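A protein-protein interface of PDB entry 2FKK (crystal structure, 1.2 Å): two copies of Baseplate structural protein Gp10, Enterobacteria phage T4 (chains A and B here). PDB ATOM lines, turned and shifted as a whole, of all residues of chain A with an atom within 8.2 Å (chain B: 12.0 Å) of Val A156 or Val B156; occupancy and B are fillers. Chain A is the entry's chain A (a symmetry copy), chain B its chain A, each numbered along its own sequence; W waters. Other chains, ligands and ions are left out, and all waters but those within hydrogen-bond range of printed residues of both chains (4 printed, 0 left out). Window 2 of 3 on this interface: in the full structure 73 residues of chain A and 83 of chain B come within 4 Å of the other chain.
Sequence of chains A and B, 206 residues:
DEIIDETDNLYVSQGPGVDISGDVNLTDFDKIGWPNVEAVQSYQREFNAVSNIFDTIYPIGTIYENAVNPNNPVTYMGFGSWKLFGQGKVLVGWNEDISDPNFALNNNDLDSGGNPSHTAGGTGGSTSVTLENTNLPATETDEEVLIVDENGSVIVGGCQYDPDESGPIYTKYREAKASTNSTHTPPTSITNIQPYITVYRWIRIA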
ATOM      1  N   LEU A 146      16.187  21.213  -2.952  1.00  0.00           N
ATOM      2  CA  LEU A 146      16.023  22.643  -2.648  1.00  0.00           C
ATOM      3  C   LEU A 146      15.252  22.802  -1.351  1.00  0.00           C
ATOM      4  O   LEU A 146      14.085  22.360  -1.261  1.00  0.00           O
ATOM      5  CB  LEU A 146      15.352  23.389  -3.785  1.00  0.00           C
ATOM      6  CG  LEU A 146      16.213  23.656  -4.922  1.00  0.00           C
ATOM      7  CD1 LEU A 146      15.392  24.216  -6.100  1.00  0.00           C
ATOM      8  CD2 LEU A 146      17.323  24.660  -4.601  1.00  0.00           C
ATOM      9  N   ILE A 147      15.903  23.406  -0.372  1.00  0.00           N
ATOM     10  CA  ILE A 147      15.355  23.550   0.968  1.00  0.00           C
ATOM     11  C   ILE A 147      15.133  25.036   1.253  1.00  0.00           C
ATOM     12  O   ILE A 147      16.049  25.863   1.046  1.00  0.00           O
ATOM     13  CB  ILE A 147      16.312  22.984   2.036  1.00  0.00           C
ATOM     14  CG1 ILE A 147      16.738  21.551   1.721  1.00  0.00           C
ATOM     15  CG2 ILE A 147      15.696  23.118   3.421  1.00  0.00           C
ATOM     16  CD1 ILE A 147      17.701  20.927   2.740  1.00  0.00           C
ATOM     17  N   SER A 153      21.284  31.074  -0.332  1.00  0.00           N
ATOM     18  CA  SER A 153      21.823  31.937  -1.367  1.00  0.00           C
ATOM     19  C   SER A 153      21.147  31.654  -2.694  1.00  0.00           C
ATOM     20  O   SER A 153      21.342  32.430  -3.653  1.00  0.00           O
ATOM     21  CB  SER A 153      23.335  31.774  -1.427  1.00  0.00           C
ATOM     22  OG  SER A 153      23.844  30.486  -1.753  1.00  0.00           O
ATOM     23  N   VAL A 154      20.383  30.613  -2.798  1.00  0.00           N
ATOM     24  CA  VAL A 154      19.754  30.210  -4.054  1.00  0.00           C
ATOM     25  C   VAL A 154      18.397  30.904  -4.189  1.00  0.00           C
ATOM     26  O   VAL A 154      17.468  30.845  -3.336  1.00  0.00           O
ATOM     27  CB  VAL A 154      19.647  28.676  -4.117  1.00  0.00           C
ATOM     28  CG1 VAL A 154      18.937  28.288  -5.418  1.00  0.00           C
ATOM     29  CG2 VAL A 154      20.995  27.984  -3.942  1.00  0.00           C
ATOM     30  N   ILE A 155      18.308  31.640  -5.315  1.00  0.00           N
ATOM     31  CA  ILE A 155      17.073  32.318  -5.523  1.00  0.00           C
ATOM     32  C   ILE A 155      16.255  31.602  -6.590  1.00  0.00           C
ATOM     33  O   ILE A 155      16.785  31.320  -7.651  1.00  0.00           O
ATOM     34  CB  ILE A 155      17.420  33.729  -5.995  1.00  0.00           C
ATOM     35  CG1 ILE A 155      18.064  34.530  -4.883  1.00  0.00           C
ATOM     36  CG2 ILE A 155      16.151  34.290  -6.536  1.00  0.00           C
ATOM     37  CD1 ILE A 155      18.578  35.903  -5.313  1.00  0.00           C
ATOM     38  N   VAL A 156      15.030  31.302  -6.259  1.00  0.00           N
ATOM     39  CA  VAL A 156      13.954  30.672  -6.960  1.00  0.00           C
ATOM     40  C   VAL A 156      12.814  31.686  -6.967  1.00  0.00           C
ATOM     41  O   VAL A 156      12.272  32.036  -8.011  1.00  0.00           O
ATOM     42  CB  VAL A 156      13.495  29.370  -6.257  1.00  0.00           C
ATOM     43  CG1 VAL A 156      12.451  28.668  -7.100  1.00  0.00           C
ATOM     44  CG2 VAL A 156      14.638  28.412  -5.962  1.00  0.00           C
ATOM     45  N   TYR A 170       5.206  21.852 -15.997  1.00  0.00           N
ATOM     46  CA  TYR A 170       3.702  21.864 -16.145  1.00  0.00           C
ATOM     47  C   TYR A 170       2.936  22.197 -14.883  1.00  0.00           C
ATOM     48  O   TYR A 170       1.807  22.656 -14.948  1.00  0.00           O
ATOM     49  CB  TYR A 170       3.310  20.479 -16.635  1.00  0.00           C
ATOM     50  CG  TYR A 170       3.651  20.342 -18.114  1.00  0.00           C
ATOM     51  CD1 TYR A 170       4.297  21.277 -18.920  1.00  0.00           C
ATOM     52  CD2 TYR A 170       3.259  19.138 -18.693  1.00  0.00           C
ATOM     53  CE1 TYR A 170       4.563  21.067 -20.250  1.00  0.00           C
ATOM     54  CE2 TYR A 170       3.527  18.941 -20.037  1.00  0.00           C
ATOM     55  CZ  TYR A 170       4.158  19.860 -20.778  1.00  0.00           C
ATOM     56  OH  TYR A 170       4.398  19.636 -22.114  1.00  0.00           O
ATOM     57  N   THR A 171       3.490  22.010 -13.696  1.00  0.00           N
ATOM     58  CA  THR A 171       2.979  22.096 -12.373  1.00  0.00           C
ATOM     59  C   THR A 171       3.680  23.300 -11.719  1.00  0.00           C
ATOM     60  O   THR A 171       4.701  23.813 -12.086  1.00  0.00           O
ATOM     61  CB  THR A 171       3.273  20.877 -11.462  1.00  0.00           C
ATOM     62  OG1 THR A 171       4.697  20.777 -11.453  1.00  0.00           O
ATOM     63  CG2 THR A 171       2.725  19.589 -12.022  1.00  0.00           C
ATOM     64  N   LYS A 172       2.937  23.719 -10.709  1.00  0.00           N
ATOM     65  CA  LYS A 172       3.580  24.579  -9.777  1.00  0.00           C
ATOM     66  C   LYS A 172       4.140  23.670  -8.676  1.00  0.00           C
ATOM     67  O   LYS A 172       4.202  22.429  -8.743  1.00  0.00           O
ATOM     68  CB  LYS A 172       2.512  25.567  -9.307  1.00  0.00           C
ATOM     69  CG  LYS A 172       1.990  26.420 -10.506  1.00  0.00           C
ATOM     70  CD  LYS A 172       0.471  26.298 -10.553  1.00  0.00           C
ATOM     71  N   TYR A 173       4.552  24.362  -7.614  1.00  0.00           N
ATOM     72  CA  TYR A 173       5.115  23.780  -6.424  1.00  0.00           C
ATOM     73  C   TYR A 173       4.458  24.362  -5.195  1.00  0.00           C
ATOM     74  O   TYR A 173       3.835  25.435  -5.241  1.00  0.00           O
ATOM     75  CB  TYR A 173       6.654  24.042  -6.377  1.00  0.00           C
ATOM     76  CG  TYR A 173       7.363  23.421  -7.543  1.00  0.00           C
ATOM     77  CD1 TYR A 173       8.008  22.189  -7.482  1.00  0.00           C
ATOM     78  CD2 TYR A 173       7.399  24.077  -8.754  1.00  0.00           C
ATOM     79  CE1 TYR A 173       8.641  21.667  -8.610  1.00  0.00           C
ATOM     80  CE2 TYR A 173       8.017  23.588  -9.872  1.00  0.00           C
ATOM     81  CZ  TYR A 173       8.645  22.377  -9.792  1.00  0.00           C
ATOM     82  OH  TYR A 173       9.279  21.828 -10.892  1.00  0.00           O
ATOM     83  N   ARG A 174       4.646  23.694  -4.108  1.00  0.00           N
ATOM     84  CA  ARG A 174       4.427  24.293  -2.803  1.00  0.00           C
ATOM     85  C   ARG A 174       5.675  24.171  -1.948  1.00  0.00           C
ATOM     86  O   ARG A 174       6.501  23.305  -2.119  1.00  0.00           O
ATOM     87  CB  ARG A 174       3.280  23.637  -2.115  1.00  0.00           C
ATOM     88  CG  ARG A 174       3.385  22.193  -1.819  1.00  0.00           C
ATOM     89  CD  ARG A 174       2.044  21.812  -1.094  1.00  0.00           C
ATOM     90  NE  ARG A 174       2.151  20.373  -0.989  1.00  0.00           N
ATOM     91  CZ  ARG A 174       2.243  19.559   0.003  1.00  0.00           C
ATOM     92  NH1 ARG A 174       2.200  20.060   1.261  1.00  0.00           N
ATOM     93  NH2 ARG A 174       2.357  18.254  -0.303  1.00  0.00           N
ATOM     94  N   GLU A 175       5.759  25.106  -1.004  1.00  0.00           N
ATOM     95  CA  GLU A 175       6.788  25.116  -0.004  1.00  0.00           C
ATOM     96  C   GLU A 175       6.249  24.417   1.233  1.00  0.00           C
ATOM     97  O   GLU A 175       5.365  24.968   1.888  1.00  0.00           O
ATOM     98  CB  GLU A 175       7.209  26.551   0.340  1.00  0.00           C
ATOM     99  CG  GLU A 175       8.052  27.349  -0.605  1.00  0.00           C
ATOM    100  CD  GLU A 175       7.877  28.828  -0.289  1.00  0.00           C
ATOM    101  OE1 GLU A 175       8.187  29.142   0.879  1.00  0.00           O
ATOM    102  OE2 GLU A 175       7.435  29.629  -1.114  1.00  0.00           O
ATOM    103  N   GLU B 144      11.152  22.863   5.245  1.00  0.00           N
ATOM    104  CA  GLU B 144      10.363  22.886   4.038  1.00  0.00           C
ATOM    105  C   GLU B 144      11.259  22.729   2.827  1.00  0.00           C
ATOM    106  O   GLU B 144      12.375  23.258   2.760  1.00  0.00           O
ATOM    107  CB  GLU B 144       9.597  24.213   3.926  1.00  0.00           C
ATOM    108  CG  GLU B 144       8.518  24.391   4.957  1.00  0.00           C
ATOM    109  CD  GLU B 144       7.706  25.659   4.750  1.00  0.00           C
ATOM    110  OE1 GLU B 144       8.045  26.514   3.924  1.00  0.00           O
ATOM    111  OE2 GLU B 144       6.668  25.741   5.491  1.00  0.00           O
ATOM    112  N   VAL B 145      10.704  22.040   1.814  1.00  0.00           N
ATOM    113  CA  VAL B 145      11.353  21.874   0.534  1.00  0.00           C
ATOM    114  C   VAL B 145      10.329  22.273  -0.533  1.00  0.00           C
ATOM    115  O   VAL B 145       9.189  22.574  -0.256  1.00  0.00           O
ATOM    116  CB  VAL B 145      11.834  20.427   0.328  1.00  0.00           C
ATOM    117  CG1 VAL B 145      12.818  20.059   1.429  1.00  0.00           C
ATOM    118  CG2 VAL B 145      10.664  19.441   0.292  1.00  0.00           C
ATOM    119  N   LEU B 146      10.733  22.286  -1.779  1.00  0.00           N
ATOM    120  CA  LEU B 146       9.843  22.529  -2.925  1.00  0.00           C
ATOM    121  C   LEU B 146       9.260  21.214  -3.405  1.00  0.00           C
ATOM    122  O   LEU B 146      10.017  20.313  -3.826  1.00  0.00           O
ATOM    123  CB  LEU B 146      10.552  23.262  -4.046  1.00  0.00           C
ATOM    124  CG  LEU B 146      10.754  24.680  -3.808  1.00  0.00           C
ATOM    125  CD1 LEU B 146      11.666  25.285  -4.894  1.00  0.00           C
ATOM    126  CD2 LEU B 146       9.443  25.471  -3.800  1.00  0.00           C
ATOM    127  N   ILE B 147       7.944  21.112  -3.326  1.00  0.00           N
ATOM    128  CA  ILE B 147       7.228  19.886  -3.645  1.00  0.00           C
ATOM    129  C   ILE B 147       6.350  20.133  -4.871  1.00  0.00           C
ATOM    130  O   ILE B 147       5.589  21.126  -4.916  1.00  0.00           O
ATOM    131  CB  ILE B 147       6.326  19.436  -2.479  1.00  0.00           C
ATOM    132  CG1 ILE B 147       7.095  19.347  -1.162  1.00  0.00           C
ATOM    133  CG2 ILE B 147       5.618  18.135  -2.830  1.00  0.00           C
ATOM    134  CD1 ILE B 147       6.254  18.913   0.047  1.00  0.00           C
ATOM    135  N   VAL B 148       6.410  19.248  -5.848  1.00  0.00           N
ATOM    136  CA  VAL B 148       5.531  19.342  -7.004  1.00  0.00           C
ATOM    137  C   VAL B 148       4.109  19.337  -6.571  1.00  0.00           C
ATOM    138  O   VAL B 148       3.724  18.435  -5.794  1.00  0.00           O
ATOM    139  CB  VAL B 148       5.832  18.158  -7.963  1.00  0.00           C
ATOM    140  CG1 VAL B 148       4.789  18.135  -9.090  1.00  0.00           C
ATOM    141  CG2 VAL B 148       7.250  18.266  -8.494  1.00  0.00           C
ATOM    142  N   ASP B 149       3.296  20.256  -7.054  1.00  0.00           N
ATOM    143  CA  ASP B 149       1.888  20.305  -6.624  1.00  0.00           C
ATOM    144  C   ASP B 149       1.042  20.946  -7.681  1.00  0.00           C
ATOM    145  O   ASP B 149       1.160  22.168  -7.888  1.00  0.00           O
ATOM    146  CB  ASP B 149       1.843  21.084  -5.327  1.00  0.00           C
ATOM    147  CG  ASP B 149       0.487  21.155  -4.672  1.00  0.00           C
ATOM    148  OD1 ASP B 149      -0.530  20.621  -5.148  1.00  0.00           O
ATOM    149  OD2 ASP B 149       0.480  21.821  -3.608  1.00  0.00           O
ATOM    150  N   GLU B 150       0.152  20.157  -8.308  1.00  0.00           N
ATOM    151  CA  GLU B 150      -0.729  20.691  -9.337  1.00  0.00           C
ATOM    152  C   GLU B 150      -1.529  21.813  -8.696  1.00  0.00           C
ATOM    153  O   GLU B 150      -1.898  22.731  -9.419  1.00  0.00           O
ATOM    154  CB  GLU B 150      -1.578  19.593  -9.969  1.00  0.00           C
ATOM    155  CG  GLU B 150      -0.898  18.500 -10.802  1.00  0.00           C
ATOM    156  CD  GLU B 150      -0.536  18.712 -12.255  1.00  0.00           C
ATOM    157  OE1 GLU B 150      -0.838  19.884 -12.597  1.00  0.00           O
ATOM    158  OE2 GLU B 150      -0.010  17.821 -12.966  1.00  0.00           O
ATOM    159  N   ASN B 151      -1.784  21.885  -7.390  1.00  0.00           N
ATOM    160  CA  ASN B 151      -2.552  22.911  -6.729  1.00  0.00           C
ATOM    161  C   ASN B 151      -1.637  23.958  -6.112  1.00  0.00           C
ATOM    162  O   ASN B 151      -2.119  24.767  -5.336  1.00  0.00           O
ATOM    163  CB  ASN B 151      -3.400  22.297  -5.620  1.00  0.00           C
ATOM    164  CG  ASN B 151      -4.538  21.406  -6.067  1.00  0.00           C
ATOM    165  OD1 ASN B 151      -4.399  20.178  -6.171  1.00  0.00           O
ATOM    166  ND2 ASN B 151      -5.731  21.959  -6.332  1.00  0.00           N
ATOM    167  N   GLY B 152      -0.353  23.915  -6.415  1.00  0.00           N
ATOM    168  CA  GLY B 152       0.668  24.776  -5.825  1.00  0.00           C
ATOM    169  C   GLY B 152       0.481  26.210  -6.286  1.00  0.00           C
ATOM    170  O   GLY B 152      -0.204  26.427  -7.284  1.00  0.00           O
ATOM    171  N   SER B 153       1.123  27.135  -5.549  1.00  0.00           N
ATOM    172  CA  SER B 153       1.096  28.528  -5.957  1.00  0.00           C
ATOM    173  C   SER B 153       2.489  28.994  -6.332  1.00  0.00           C
ATOM    174  O   SER B 153       2.630  30.102  -6.891  1.00  0.00           O
ATOM    175  CB  SER B 153       0.469  29.367  -4.853  1.00  0.00           C
ATOM    176  OG  SER B 153       1.126  29.391  -3.592  1.00  0.00           O
ATOM    177  N   VAL B 154       3.499  28.228  -6.063  1.00  0.00           N
ATOM    178  CA  VAL B 154       4.884  28.623  -6.309  1.00  0.00           C
ATOM    179  C   VAL B 154       5.283  28.220  -7.730  1.00  0.00           C
ATOM    180  O   VAL B 154       5.198  27.051  -8.200  1.00  0.00           O
ATOM    181  CB  VAL B 154       5.802  28.009  -5.237  1.00  0.00           C
ATOM    182  CG1 VAL B 154       7.251  28.396  -5.552  1.00  0.00           C
ATOM    183  CG2 VAL B 154       5.380  28.379  -3.819  1.00  0.00           C
ATOM    184  N   ILE B 155       5.700  29.272  -8.463  1.00  0.00           N
ATOM    185  CA  ILE B 155       6.096  28.985  -9.801  1.00  0.00           C
ATOM    186  C   ILE B 155       7.615  29.013  -9.916  1.00  0.00           C
ATOM    187  O   ILE B 155       8.223  29.972  -9.474  1.00  0.00           O
ATOM    188  CB  ILE B 155       5.489  30.075 -10.682  1.00  0.00           C
ATOM    189  CG1 ILE B 155       3.981  29.948 -10.740  1.00  0.00           C
ATOM    190  CG2 ILE B 155       6.191  29.963 -11.991  1.00  0.00           C
ATOM    191  CD1 ILE B 155       3.282  31.087 -11.480  1.00  0.00           C
ATOM    192  N   VAL B 156       8.162  27.959 -10.456  1.00  0.00           N
ATOM    193  CA  VAL B 156       9.514  27.608 -10.763  1.00  0.00           C
ATOM    194  C   VAL B 156       9.546  27.361 -12.269  1.00  0.00           C
ATOM    195  O   VAL B 156      10.340  27.945 -12.999  1.00  0.00           O
ATOM    196  CB  VAL B 156       9.962  26.331 -10.010  1.00  0.00           C
ATOM    197  CG1 VAL B 156      11.433  26.073 -10.259  1.00  0.00           C
ATOM    198  CG2 VAL B 156       9.703  26.393  -8.513  1.00  0.00           C
ATOM    199  N   TYR B 170      24.761  25.735 -10.861  1.00  0.00           N
ATOM    200  CA  TYR B 170      25.608  24.992 -11.869  1.00  0.00           C
ATOM    201  C   TYR B 170      24.952  23.773 -12.480  1.00  0.00           C
ATOM    202  O   TYR B 170      25.315  23.356 -13.568  1.00  0.00           O
ATOM    203  CB  TYR B 170      26.878  24.583 -11.140  1.00  0.00           C
ATOM    204  CG  TYR B 170      27.788  25.795 -10.977  1.00  0.00           C
ATOM    205  CD1 TYR B 170      27.514  27.110 -11.344  1.00  0.00           C
ATOM    206  CD2 TYR B 170      29.023  25.521 -10.394  1.00  0.00           C
ATOM    207  CE1 TYR B 170      28.400  28.143 -11.158  1.00  0.00           C
ATOM    208  CE2 TYR B 170      29.910  26.570 -10.219  1.00  0.00           C
ATOM    209  CZ  TYR B 170      29.607  27.824 -10.577  1.00  0.00           C
ATOM    210  OH  TYR B 170      30.517  28.840 -10.398  1.00  0.00           O
ATOM    211  N   THR B 171      23.967  23.155 -11.848  1.00  0.00           N
ATOM    212  CA  THR B 171      23.275  21.940 -12.102  1.00  0.00           C
ATOM    213  C   THR B 171      21.835  22.335 -12.474  1.00  0.00           C
ATOM    214  O   THR B 171      21.301  23.382 -12.231  1.00  0.00           O
ATOM    215  CB  THR B 171      23.161  20.972 -10.897  1.00  0.00           C
ATOM    216  OG1 THR B 171      22.497  21.736  -9.891  1.00  0.00           O
ATOM    217  CG2 THR B 171      24.505  20.564 -10.351  1.00  0.00           C
ATOM    218  N   LYS B 172      21.295  21.345 -13.163  1.00  0.00           N
ATOM    219  CA  LYS B 172      19.878  21.371 -13.284  1.00  0.00           C
ATOM    220  C   LYS B 172      19.335  20.539 -12.117  1.00  0.00           C
ATOM    221  O   LYS B 172      20.014  20.137 -11.155  1.00  0.00           O
ATOM    222  CB  LYS B 172      19.563  20.808 -14.671  1.00  0.00           C
ATOM    223  CG  LYS B 172      20.184  21.713 -15.782  1.00  0.00           C
ATOM    224  CD  LYS B 172      21.040  20.835 -16.689  1.00  0.00           C
ATOM    225  N   TYR B 173      18.036  20.273 -12.251  1.00  0.00           N
ATOM    226  CA  TYR B 173      17.255  19.505 -11.317  1.00  0.00           C
ATOM    227  C   TYR B 173      16.435  18.468 -12.047  1.00  0.00           C
ATOM    228  O   TYR B 173      16.203  18.566 -13.263  1.00  0.00           O
ATOM    229  CB  TYR B 173      16.314  20.448 -10.502  1.00  0.00           C
ATOM    230  CG  TYR B 173      17.087  21.453  -9.701  1.00  0.00           C
ATOM    231  CD1 TYR B 173      17.382  21.294  -8.351  1.00  0.00           C
ATOM    232  CD2 TYR B 173      17.542  22.606 -10.302  1.00  0.00           C
ATOM    233  CE1 TYR B 173      18.114  22.268  -7.669  1.00  0.00           C
ATOM    234  CE2 TYR B 173      18.257  23.577  -9.654  1.00  0.00           C
ATOM    235  CZ  TYR B 173      18.536  23.404  -8.328  1.00  0.00           C
ATOM    236  OH  TYR B 173      19.263  24.346  -7.622  1.00  0.00           O
ATOM    237  N   ARG B 174      15.959  17.527 -11.305  1.00  0.00           N
ATOM    238  CA  ARG B 174      14.859  16.691 -11.754  1.00  0.00           C
ATOM    239  C   ARG B 174      13.719  16.735 -10.753  1.00  0.00           C
ATOM    240  O   ARG B 174      13.885  16.990  -9.584  1.00  0.00           O
ATOM    241  CB  ARG B 174      15.315  15.285 -11.937  1.00  0.00           C
ATOM    242  CG  ARG B 174      15.834  14.567 -10.754  1.00  0.00           C
ATOM    243  CD  ARG B 174      16.215  13.131 -11.265  1.00  0.00           C
ATOM    244  NE  ARG B 174      16.859  12.554 -10.106  1.00  0.00           N
ATOM    245  CZ  ARG B 174      16.573  11.571  -9.327  1.00  0.00           C
ATOM    246  NH1 ARG B 174      15.470  10.830  -9.593  1.00  0.00           N
ATOM    247  NH2 ARG B 174      17.424  11.347  -8.309  1.00  0.00           N
ATOM    248  N   GLU B 175      12.533  16.464 -11.296  1.00  0.00           N
ATOM    249  CA  GLU B 175      11.332  16.329 -10.522  1.00  0.00           C
ATOM    250  C   GLU B 175      11.134  14.853 -10.215  1.00  0.00           C
ATOM    251  O   GLU B 175      10.834  14.092 -11.133  1.00  0.00           O
ATOM    252  CB  GLU B 175      10.120  16.879 -11.283  1.00  0.00           C
ATOM    253  CG  GLU B 175       9.915  18.353 -11.434  1.00  0.00           C
ATOM    254  CD  GLU B 175       8.995  18.603 -12.622  1.00  0.00           C
ATOM    255  OE1 GLU B 175       7.877  18.056 -12.527  1.00  0.00           O
ATOM    256  OE2 GLU B 175       9.349  19.261 -13.600  1.00  0.00           O
ATOM    257  N   ALA B 176      11.298  14.446  -8.949  1.00  0.00           N
ATOM    258  CA  ALA B 176      11.189  13.031  -8.629  1.00  0.00           C
ATOM    259  C   ALA B 176      11.032  12.906  -7.126  1.00  0.00           C
ATOM    260  O   ALA B 176      11.358  13.791  -6.354  1.00  0.00           O
ATOM    261  CB  ALA B 176      12.425  12.247  -9.052  1.00  0.00           C
HETATM  262  O   HOH W   1      -0.225  23.201 -11.322  1.00  0.00           O
HETATM  263  O   HOH W   2       2.064  18.289  -3.465  1.00  0.00           O
HETATM  264  O   HOH W   3       6.139  25.722 -11.854  1.00  0.00           O
HETATM  265  O   HOH W   4      12.998  20.519  -3.391  1.00  0.00           O
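Of chain B, only Val B156 comes within 4 Å of Val A156.
Of chain A, only Val A156 and Tyr A173 come within 4 Å of Val B156.
No residue of chain B comes within 4 Å of Ile A155.
Of the printed residues of chain A, Gly B152 touches Lys A172 (3.3 Å) and Tyr A173 (3.3 Å).
Printed residues of chain A within 4 Å of Ser B153: Tyr A173.
Of the printed residues of chain B, Glu A175 touches Glu B144, Val B145, Leu B146 and Val B154.
Printed residues of chain A within 4 Å of Glu B144: Ile A147 (3.4 Å) and Glu A175 (3.7 Å).
Printed residues of chain B within 4 Å of Tyr A173: Ile B147, Val B148, Gly B152, Ser B153, Val B154, Val B156 and Glu B175.
Tyr B170 touches none of the printed residues of chain A.
The nearest residue of chain B that does not touch Val A156 is Leu B146 (4.1 Å).
Leu A146 touches Tyr B173, but with the chains exchanged Tyr A173 does not touch Leu B146 (4.1 Å).
Val A156 touches its own counterpart, Val B156.
Tyr A173 touches Ile B147, but with the chains exchanged Ile A147 does not touch Tyr B173 (7.7 Å).
Arg A174 touches Leu B146, but with the chains exchanged Leu A146 does not touch Arg B174 (8.2 Å).
Positions printed for both chains: 146, 147, 153, 154, 155, 156, 170, 171, 172, 173, 174 and 175.
Of the 26 pairs that touch across the chains among the printed residues, 2 have their exchanged pair printed and touching as well.
Of the 20 printed residues of chain B, 13 touch a printed residue of chain A.
Hydrophobic or aromatic side chains of chain B within 4 Å of the printed part of chain A: Val B145, Leu B146, Ile B147, Val B148, Val B154, Val B156 and Tyr B173.
Printed residues of chain A that touch a printed residue of chain B: Leu A146, Ile A147, Val A156, Thr A171, Lys A172, Tyr A173, Arg A174 and Glu A175.
Among the printed residues, Asp or Glu carboxylates within 4 Å of a Lys or Arg side-chain nitrogen of the other chain: Arg A174 with Asp B149.
O of Val B145 sits close to O of Arg A174, 3.4 Å away.
The backbone NH (N) of Leu B146 lies within hydrogen-bond range of the backbone carbonyl oxygen (O) of Leu A146 (3.4 Å).
NE of Arg A174 is in salt-bridge range of OD2 of Asp B149 (3.4 Å).
O of Val B154 sits at hydrogen-bond distance from N of Tyr A173 (2.8 Å).
The backbone carbonyl oxygen (O) of Ile B147 is in hydrogen-bond range of the backbone NH (N) of Arg A174, 2.9 Å away.
The backbone carbonyl oxygen of Tyr A173 is in hydrogen-bond range of the backbone NH of Ser B153 (3.2 Å).
N of Asp B149 is in hydrogen-bond range of O of Lys A172 (2.9 Å).
OD1 of Asp B149 is in hydrogen-bond range of N of Asn B151, at 2.9 Å.
Water W3 lies within hydrogen-bond range of the backbone carbonyl oxygen of Thr A171 and the backbone NH of Val B156.
Water W1 bridges O of Glu B150 and N of Lys A172.
Water W2 lies within hydrogen-bond range of the backbone carbonyl oxygen (O) of Val B148 (2.9 Å) and the guanidinium group (NH2) of Arg A174 (3.2 Å).
Water W4 lies within hydrogen-bond range of the backbone carbonyl oxygen of Leu A146 (3.0 Å) and the backbone carbonyl oxygen of Leu B146 (3.0 Å).
Among the printed residues, pairs that only touch across the chains: Tyr A173 with Ile B147, Lys A172 with Val B154, Tyr A173 with Val B156, Tyr A173 with Gly B152, Leu A146 with Val B145, Lys A172 with Gly B152, Thr A171 with Glu B150, Ile A147 with Glu B144, Glu A175 with Val B145, Arg A174 with Leu B146, Thr A171 with Val B148, Tyr A173 with Glu B175, Leu A146 with Tyr B173, Glu A175 with Val B154, Tyr A173 with Val B148, Glu A175 with Glu B144, Lys A172 with Val B148, Val A156 with Val B156 and Glu A175 with Leu B146.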
